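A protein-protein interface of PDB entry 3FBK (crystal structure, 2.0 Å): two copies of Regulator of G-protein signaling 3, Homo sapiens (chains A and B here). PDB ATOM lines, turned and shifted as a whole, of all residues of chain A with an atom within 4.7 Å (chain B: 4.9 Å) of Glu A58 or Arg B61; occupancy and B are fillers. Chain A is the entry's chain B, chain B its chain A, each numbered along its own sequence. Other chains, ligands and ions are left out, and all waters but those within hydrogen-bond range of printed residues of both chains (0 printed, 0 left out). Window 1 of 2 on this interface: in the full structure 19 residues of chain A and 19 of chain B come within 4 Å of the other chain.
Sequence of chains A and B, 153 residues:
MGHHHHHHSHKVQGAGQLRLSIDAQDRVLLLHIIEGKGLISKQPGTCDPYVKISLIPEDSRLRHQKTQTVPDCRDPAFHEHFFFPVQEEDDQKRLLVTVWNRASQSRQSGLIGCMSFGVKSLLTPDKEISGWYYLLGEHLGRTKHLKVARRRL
The side-chain amino group (NZ) of Lys B52 lies within salt-bridge range of the side-chain carboxylate (OD2) of Asp A59, 2.8 Å away. The guanidinium group (NH1) of Arg A61 is in salt-bridge range of the side-chain carboxylate (OD2) of Asp B59, at 2.9 Å. The backbone carbonyl oxygen of Ser B60 lies within hydrogen-bond range of the guanidinium group of Arg A61 (3.3 Å). O of Glu A58 sits at hydrogen-bond distance from NH2 of Arg B61, 3.0 Å away. NH1 of Arg B61 lies within salt-bridge range of OD2 of Asp A59, at 3.0 Å. The backbone carbonyl oxygen of Ser A60 lies within hydrogen-bond range of the guanidinium group of Arg B61. The side-chain amino group of Lys A93 lies within hydrogen-bond range of the backbone carbonyl oxygen of Arg B107. NE of Arg A61 lies close to NE of Arg B61.
Among the printed residues, pairs that only touch across the chains: Glu A58 with Trp B100, Glu A58 with Arg B107, Asp A59 with Trp B100 and Arg A63 with Arg B107.
The side-chain hydroxyl (OG) of Ser B60 is in hydrogen-bond range of the backbone NH (N) of Leu B62 (3.4 Å). The backbone carbonyl oxygen of Ser B60 is in hydrogen-bond range of a ring nitrogen (NE2) of His B64 (3.3 Å). OE2 of Glu A58 is in salt-bridge range of NH2 of Arg A63 (3.0 Å). OE2 of Glu A58 is in salt-bridge range of NZ of Lys A93. NH1 of Arg A63 is in salt-bridge range of OD1 of Asp A90, 2.6 Å away. The side-chain carboxylate (OD2) of Asp A90 is in salt-bridge range of the side-chain amino group (NZ) of Lys A93 (3.0 Å).
Of the 10 printed residues of chain A, 6 touch a printed residue of chain B. Printed residues of chain A that touch a printed residue of chain B: Glu A58, Asp A59, Ser A60, Arg A61, Arg A63 and Lys A93. Of the 9 printed residues of chain B, 6 touch a printed residue of chain A. Hydrophobic or aromatic side chains of chain B that line the printed part of chain A: Trp B100. Along chain B the printed residues that touch a printed residue of chain A span positions 52 to 107. Among the printed residues, 12 pairs touch across the chains. Among the printed residues, Asp or Glu carboxylates within 4 Å of a Lys or Arg side-chain nitrogen of the other chain: Asp A59 with Lys B52, Asp A59 with Arg B61 and Arg A61 with Asp B59.
Of the printed residues of chain B, Glu A58 touches Arg B61 (3.0 Å), Trp B100 (3.6 Å) and Arg B107 (3.6 Å). Printed residues of chain B within 4 Å of Asp A59: Lys B52 (2.8 Å), Arg B61 (3.0 Å) and Trp B100 (3.4 Å). Of the printed residues of chain A, Lys B52 touches Asp A59. Of chain A, only Glu A58 (3.0 Å), Asp A59 (3.0 Å), Ser A60 (2.8 Å) and Arg A61 (3.0 Å) come within 4 Å of Arg B61. Printed residues of chain A within 4 Å of Trp B100: Glu A58 and Asp A59. The nearest printed residue of chain B that does not touch Lys A93 is Trp B100 (7.5 Å).
Asp A59 touches Arg B61, and with the chains exchanged Arg A61 touches Asp B59. Ser A60 touches Arg B61, and with the chains exchanged Arg A61 touches Ser B60. Arg A61 touches its own counterpart, Arg B61. Of the 12 pairs that touch across the chains among the printed residues, 5 have their exchanged pair printed and touching as well.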
ATOM      1  N   LEU A  55     -25.611  28.785   3.218  1.00  0.00           N
ATOM      2  CA  LEU A  55     -26.105  27.902   2.178  1.00  0.00           C
ATOM      3  C   LEU A  55     -27.213  27.067   2.784  1.00  0.00           C
ATOM      4  O   LEU A  55     -27.155  26.730   3.967  1.00  0.00           O
ATOM      5  CB  LEU A  55     -25.006  26.972   1.686  1.00  0.00           C
ATOM      6  CG  LEU A  55     -23.809  27.577   0.961  1.00  0.00           C
ATOM      7  CD1 LEU A  55     -22.926  26.430   0.485  1.00  0.00           C
ATOM      8  CD2 LEU A  55     -24.271  28.421  -0.223  1.00  0.00           C
ATOM      9  N   ILE A  56     -28.210  26.723   1.972  1.00  0.00           N
ATOM     10  CA  ILE A  56     -29.321  25.896   2.437  1.00  0.00           C
ATOM     11  C   ILE A  56     -29.719  24.872   1.377  1.00  0.00           C
ATOM     12  O   ILE A  56     -29.625  25.134   0.177  1.00  0.00           O
ATOM     13  CB  ILE A  56     -30.576  26.738   2.777  1.00  0.00           C
ATOM     14  CG1 ILE A  56     -31.056  27.497   1.535  1.00  0.00           C
ATOM     15  CG2 ILE A  56     -30.255  27.711   3.910  1.00  0.00           C
ATOM     16  CD1 ILE A  56     -32.315  28.336   1.780  1.00  0.00           C
ATOM     17  N   PRO A  57     -30.131  23.670   1.809  1.00  0.00           N
ATOM     18  CA  PRO A  57     -30.224  23.294   3.224  1.00  0.00           C
ATOM     19  C   PRO A  57     -28.871  22.780   3.711  1.00  0.00           C
ATOM     20  O   PRO A  57     -28.113  22.177   2.948  1.00  0.00           O
ATOM     21  CB  PRO A  57     -31.304  22.217   3.229  1.00  0.00           C
ATOM     22  CG  PRO A  57     -31.092  21.534   1.911  1.00  0.00           C
ATOM     23  CD  PRO A  57     -30.823  22.688   0.954  1.00  0.00           C
ATOM     24  N   GLU A  58     -28.554  23.044   4.973  1.00  0.00           N
ATOM     25  CA  GLU A  58     -27.283  22.604   5.538  1.00  0.00           C
ATOM     26  C   GLU A  58     -27.364  22.636   7.052  1.00  0.00           C
ATOM     27  O   GLU A  58     -27.634  23.675   7.648  1.00  0.00           O
ATOM     28  CB  GLU A  58     -26.139  23.513   5.077  1.00  0.00           C
ATOM     29  CG  GLU A  58     -24.757  22.906   5.299  1.00  0.00           C
ATOM     30  CD  GLU A  58     -23.632  23.776   4.764  1.00  0.00           C
ATOM     31  OE1 GLU A  58     -23.239  24.738   5.459  1.00  0.00           O
ATOM     32  OE2 GLU A  58     -23.150  23.502   3.642  1.00  0.00           O
ATOM     33  N   ASP A  59     -27.129  21.489   7.673  1.00  0.00           N
ATOM     34  CA  ASP A  59     -27.188  21.399   9.120  1.00  0.00           C
ATOM     35  C   ASP A  59     -25.844  21.764   9.751  1.00  0.00           C
ATOM     36  O   ASP A  59     -25.178  20.915  10.335  1.00  0.00           O
ATOM     37  CB  ASP A  59     -27.593  19.985   9.535  1.00  0.00           C
ATOM     38  CG  ASP A  59     -27.905  19.886  11.008  1.00  0.00           C
ATOM     39  OD1 ASP A  59     -28.090  18.759  11.496  1.00  0.00           O
ATOM     40  OD2 ASP A  59     -27.982  20.941  11.677  1.00  0.00           O
ATOM     41  N   SER A  60     -25.454  23.027   9.622  1.00  0.00           N
ATOM     42  CA  SER A  60     -24.198  23.517  10.179  1.00  0.00           C
ATOM     43  C   SER A  60     -24.096  25.019   9.955  1.00  0.00           C
ATOM     44  O   SER A  60     -24.577  25.533   8.943  1.00  0.00           O
ATOM     45  CB  SER A  60     -23.007  22.832   9.511  1.00  0.00           C
ATOM     46  OG  SER A  60     -21.783  23.334  10.037  1.00  0.00           O
ATOM     47  N   ARG A  61     -23.472  25.724  10.896  1.00  0.00           N
ATOM     48  CA  ARG A  61     -23.318  27.171  10.775  1.00  0.00           C
ATOM     49  C   ARG A  61     -21.864  27.581  10.603  1.00  0.00           C
ATOM     50  O   ARG A  61     -21.555  28.771  10.512  1.00  0.00           O
ATOM     51  CB  ARG A  61     -23.894  27.874  12.004  1.00  0.00           C
ATOM     52  CG  ARG A  61     -25.396  27.757  12.135  1.00  0.00           C
ATOM     53  CD  ARG A  61     -25.951  28.900  12.966  1.00  0.00           C
ATOM     54  NE  ARG A  61     -27.411  28.939  12.945  1.00  0.00           N
ATOM     55  CZ  ARG A  61     -28.135  29.935  13.444  1.00  0.00           C
ATOM     56  NH1 ARG A  61     -27.532  30.974  14.001  1.00  0.00           N
ATOM     57  NH2 ARG A  61     -29.460  29.894  13.382  1.00  0.00           N
ATOM     58  N   ARG A  63     -20.064  27.603   8.124  1.00  0.00           N
ATOM     59  CA  ARG A  63     -19.840  28.373   6.905  1.00  0.00           C
ATOM     60  C   ARG A  63     -20.559  29.718   6.867  1.00  0.00           C
ATOM     61  O   ARG A  63     -20.365  30.507   5.933  1.00  0.00           O
ATOM     62  CB  ARG A  63     -20.244  27.547   5.680  1.00  0.00           C
ATOM     63  CG  ARG A  63     -19.522  26.211   5.598  1.00  0.00           C
ATOM     64  CD  ARG A  63     -20.079  25.335   4.486  1.00  0.00           C
ATOM     65  NE  ARG A  63     -19.632  25.757   3.163  1.00  0.00           N
ATOM     66  CZ  ARG A  63     -19.893  25.085   2.045  1.00  0.00           C
ATOM     67  NH1 ARG A  63     -19.444  25.527   0.877  1.00  0.00           N
ATOM     68  NH2 ARG A  63     -20.609  23.969   2.100  1.00  0.00           N
ATOM     69  N   ASP A  90     -22.008  21.134  -3.195  1.00  0.00           N
ATOM     70  CA  ASP A  90     -22.866  22.259  -2.836  1.00  0.00           C
ATOM     71  C   ASP A  90     -23.725  22.744  -4.004  1.00  0.00           C
ATOM     72  O   ASP A  90     -24.586  23.598  -3.823  1.00  0.00           O
ATOM     73  CB  ASP A  90     -22.010  23.438  -2.351  1.00  0.00           C
ATOM     74  CG  ASP A  90     -21.270  23.151  -1.053  1.00  0.00           C
ATOM     75  OD1 ASP A  90     -20.194  23.760  -0.856  1.00  0.00           O
ATOM     76  OD2 ASP A  90     -21.759  22.348  -0.228  1.00  0.00           O
ATOM     77  N   LYS A  93     -27.413  23.241  -3.586  1.00  0.00           N
ATOM     78  CA  LYS A  93     -27.874  24.071  -2.477  1.00  0.00           C
ATOM     79  C   LYS A  93     -28.132  25.477  -2.994  1.00  0.00           C
ATOM     80  O   LYS A  93     -27.867  25.783  -4.161  1.00  0.00           O
ATOM     81  CB  LYS A  93     -26.832  24.132  -1.364  1.00  0.00           C
ATOM     82  CG  LYS A  93     -26.526  22.790  -0.699  1.00  0.00           C
ATOM     83  CD  LYS A  93     -25.447  22.957   0.362  1.00  0.00           C
ATOM     84  CE  LYS A  93     -25.028  21.614   0.951  1.00  0.00           C
ATOM     85  NZ  LYS A  93     -23.860  21.767   1.879  1.00  0.00           N
ATOM     86  N   LYS B  52     -33.965  16.702  13.854  1.00  0.00           N
ATOM     87  CA  LYS B  52     -33.490  17.913  14.511  1.00  0.00           C
ATOM     88  C   LYS B  52     -34.678  18.828  14.771  1.00  0.00           C
ATOM     89  O   LYS B  52     -35.490  19.058  13.881  1.00  0.00           O
ATOM     90  CB  LYS B  52     -32.479  18.627  13.618  1.00  0.00           C
ATOM     91  CG  LYS B  52     -31.737  19.762  14.295  1.00  0.00           C
ATOM     92  CD  LYS B  52     -30.941  20.543  13.267  1.00  0.00           C
ATOM     93  CE  LYS B  52     -29.906  21.440  13.915  1.00  0.00           C
ATOM     94  NZ  LYS B  52     -28.698  20.677  14.355  1.00  0.00           N
ATOM     95  N   ASP B  59     -31.836  33.295  14.492  1.00  0.00           N
ATOM     96  CA  ASP B  59     -30.426  33.289  14.155  1.00  0.00           C
ATOM     97  C   ASP B  59     -29.587  32.767  15.319  1.00  0.00           C
ATOM     98  O   ASP B  59     -28.814  33.514  15.921  1.00  0.00           O
ATOM     99  CB  ASP B  59     -29.977  34.700  13.772  1.00  0.00           C
ATOM    100  CG  ASP B  59     -28.582  34.726  13.193  1.00  0.00           C
ATOM    101  OD1 ASP B  59     -28.047  35.836  12.988  1.00  0.00           O
ATOM    102  OD2 ASP B  59     -28.029  33.633  12.930  1.00  0.00           O
ATOM    103  N   SER B  60     -29.747  31.485  15.632  1.00  0.00           N
ATOM    104  CA  SER B  60     -29.003  30.849  16.712  1.00  0.00           C
ATOM    105  C   SER B  60     -29.328  29.366  16.743  1.00  0.00           C
ATOM    106  O   SER B  60     -30.450  28.969  16.435  1.00  0.00           O
ATOM    107  CB  SER B  60     -29.369  31.471  18.060  1.00  0.00           C
ATOM    108  OG  SER B  60     -28.658  30.841  19.115  1.00  0.00           O
ATOM    109  N   ARG B  61     -28.352  28.547  17.116  1.00  0.00           N
ATOM    110  CA  ARG B  61     -28.566  27.103  17.181  1.00  0.00           C
ATOM    111  C   ARG B  61     -28.492  26.577  18.604  1.00  0.00           C
ATOM    112  O   ARG B  61     -28.620  25.372  18.830  1.00  0.00           O
ATOM    113  CB  ARG B  61     -27.536  26.367  16.325  1.00  0.00           C
ATOM    114  CG  ARG B  61     -27.684  26.607  14.834  1.00  0.00           C
ATOM    115  CD  ARG B  61     -27.066  25.468  14.046  1.00  0.00           C
ATOM    116  NE  ARG B  61     -27.369  25.564  12.622  1.00  0.00           N
ATOM    117  CZ  ARG B  61     -27.106  24.604  11.742  1.00  0.00           C
ATOM    118  NH1 ARG B  61     -26.536  23.474  12.145  1.00  0.00           N
ATOM    119  NH2 ARG B  61     -27.412  24.771  10.461  1.00  0.00           N
ATOM    120  N   LEU B  62     -28.289  27.477  19.560  1.00  0.00           N
ATOM    121  CA  LEU B  62     -28.194  27.080  20.956  1.00  0.00           C
ATOM    122  C   LEU B  62     -29.404  26.278  21.420  1.00  0.00           C
ATOM    123  O   LEU B  62     -29.276  25.402  22.266  1.00  0.00           O
ATOM    124  CB  LEU B  62     -28.020  28.314  21.847  1.00  0.00           C
ATOM    125  CG  LEU B  62     -26.714  29.099  21.666  1.00  0.00           C
ATOM    126  CD1 LEU B  62     -26.739  30.353  22.533  1.00  0.00           C
ATOM    127  CD2 LEU B  62     -25.532  28.217  22.037  1.00  0.00           C
ATOM    128  N   ARG B  63     -30.573  26.566  20.857  1.00  0.00           N
ATOM    129  CA  ARG B  63     -31.790  25.865  21.254  1.00  0.00           C
ATOM    130  C   ARG B  63     -32.076  24.594  20.467  1.00  0.00           C
ATOM    131  O   ARG B  63     -33.005  23.850  20.794  1.00  0.00           O
ATOM    132  CB  ARG B  63     -32.995  26.809  21.158  1.00  0.00           C
ATOM    133  CG  ARG B  63     -32.830  28.077  21.981  1.00  0.00           C
ATOM    134  CD  ARG B  63     -33.948  29.069  21.719  1.00  0.00           C
ATOM    135  NE  ARG B  63     -35.195  28.708  22.388  1.00  0.00           N
ATOM    136  CZ  ARG B  63     -36.278  29.479  22.400  1.00  0.00           C
ATOM    137  NH1 ARG B  63     -37.373  29.087  23.037  1.00  0.00           N
ATOM    138  NH2 ARG B  63     -36.264  30.646  21.768  1.00  0.00           N
ATOM    139  N   HIS B  64     -31.279  24.330  19.438  1.00  0.00           N
ATOM    140  CA  HIS B  64     -31.484  23.138  18.620  1.00  0.00           C
ATOM    141  C   HIS B  64     -31.262  21.829  19.388  1.00  0.00           C
ATOM    142  O   HIS B  64     -30.391  21.748  20.246  1.00  0.00           O
ATOM    143  CB  HIS B  64     -30.557  23.174  17.401  1.00  0.00           C
ATOM    144  CG  HIS B  64     -30.865  24.279  16.436  1.00  0.00           C
ATOM    145  ND1 HIS B  64     -30.323  24.332  15.170  1.00  0.00           N
ATOM    146  CD2 HIS B  64     -31.663  25.368  16.549  1.00  0.00           C
ATOM    147  CE1 HIS B  64     -30.775  25.404  14.542  1.00  0.00           C
ATOM    148  NE2 HIS B  64     -31.590  26.050  15.357  1.00  0.00           N
ATOM    149  N   TRP B 100     -32.847  14.547   8.811  1.00  0.00           N
ATOM    150  CA  TRP B 100     -31.620  14.676   8.033  1.00  0.00           C
ATOM    151  C   TRP B 100     -31.002  13.307   7.784  1.00  0.00           C
ATOM    152  O   TRP B 100     -31.148  12.396   8.591  1.00  0.00           O
ATOM    153  CB  TRP B 100     -30.598  15.531   8.792  1.00  0.00           C
ATOM    154  CG  TRP B 100     -30.955  16.961   8.950  1.00  0.00           C
ATOM    155  CD1 TRP B 100     -31.662  17.527   9.975  1.00  0.00           C
ATOM    156  CD2 TRP B 100     -30.616  18.026   8.061  1.00  0.00           C
ATOM    157  NE1 TRP B 100     -31.782  18.882   9.778  1.00  0.00           N
ATOM    158  CE2 TRP B 100     -31.151  19.215   8.606  1.00  0.00           C
ATOM    159  CE3 TRP B 100     -29.915  18.092   6.846  1.00  0.00           C
ATOM    160  CZ2 TRP B 100     -31.001  20.460   7.986  1.00  0.00           C
ATOM    161  CZ3 TRP B 100     -29.767  19.334   6.228  1.00  0.00           C
ATOM    162  CH2 TRP B 100     -30.312  20.499   6.799  1.00  0.00           C
ATOM    163  N   ARG B 107     -21.766  19.282   6.593  1.00  0.00           N
ATOM    164  CA  ARG B 107     -22.159  20.026   5.400  1.00  0.00           C
ATOM    165  C   ARG B 107     -22.665  19.126   4.271  1.00  0.00           C
ATOM    166  O   ARG B 107     -23.351  19.595   3.364  1.00  0.00           O
ATOM    167  CB  ARG B 107     -21.000  20.882   4.884  1.00  0.00           C
ATOM    168  CG  ARG B 107     -19.861  20.092   4.268  1.00  0.00           C
ATOM    169  CD  ARG B 107     -18.873  21.001   3.551  1.00  0.00           C
ATOM    170  NE  ARG B 107     -18.251  21.976   4.444  1.00  0.00           N
ATOM    171  CZ  ARG B 107     -17.375  22.895   4.047  1.00  0.00           C
ATOM    172  NH1 ARG B 107     -17.020  22.968   2.766  1.00  0.00           N
ATOM    173  NH2 ARG B 107     -16.854  23.738   4.928  1.00  0.00           N
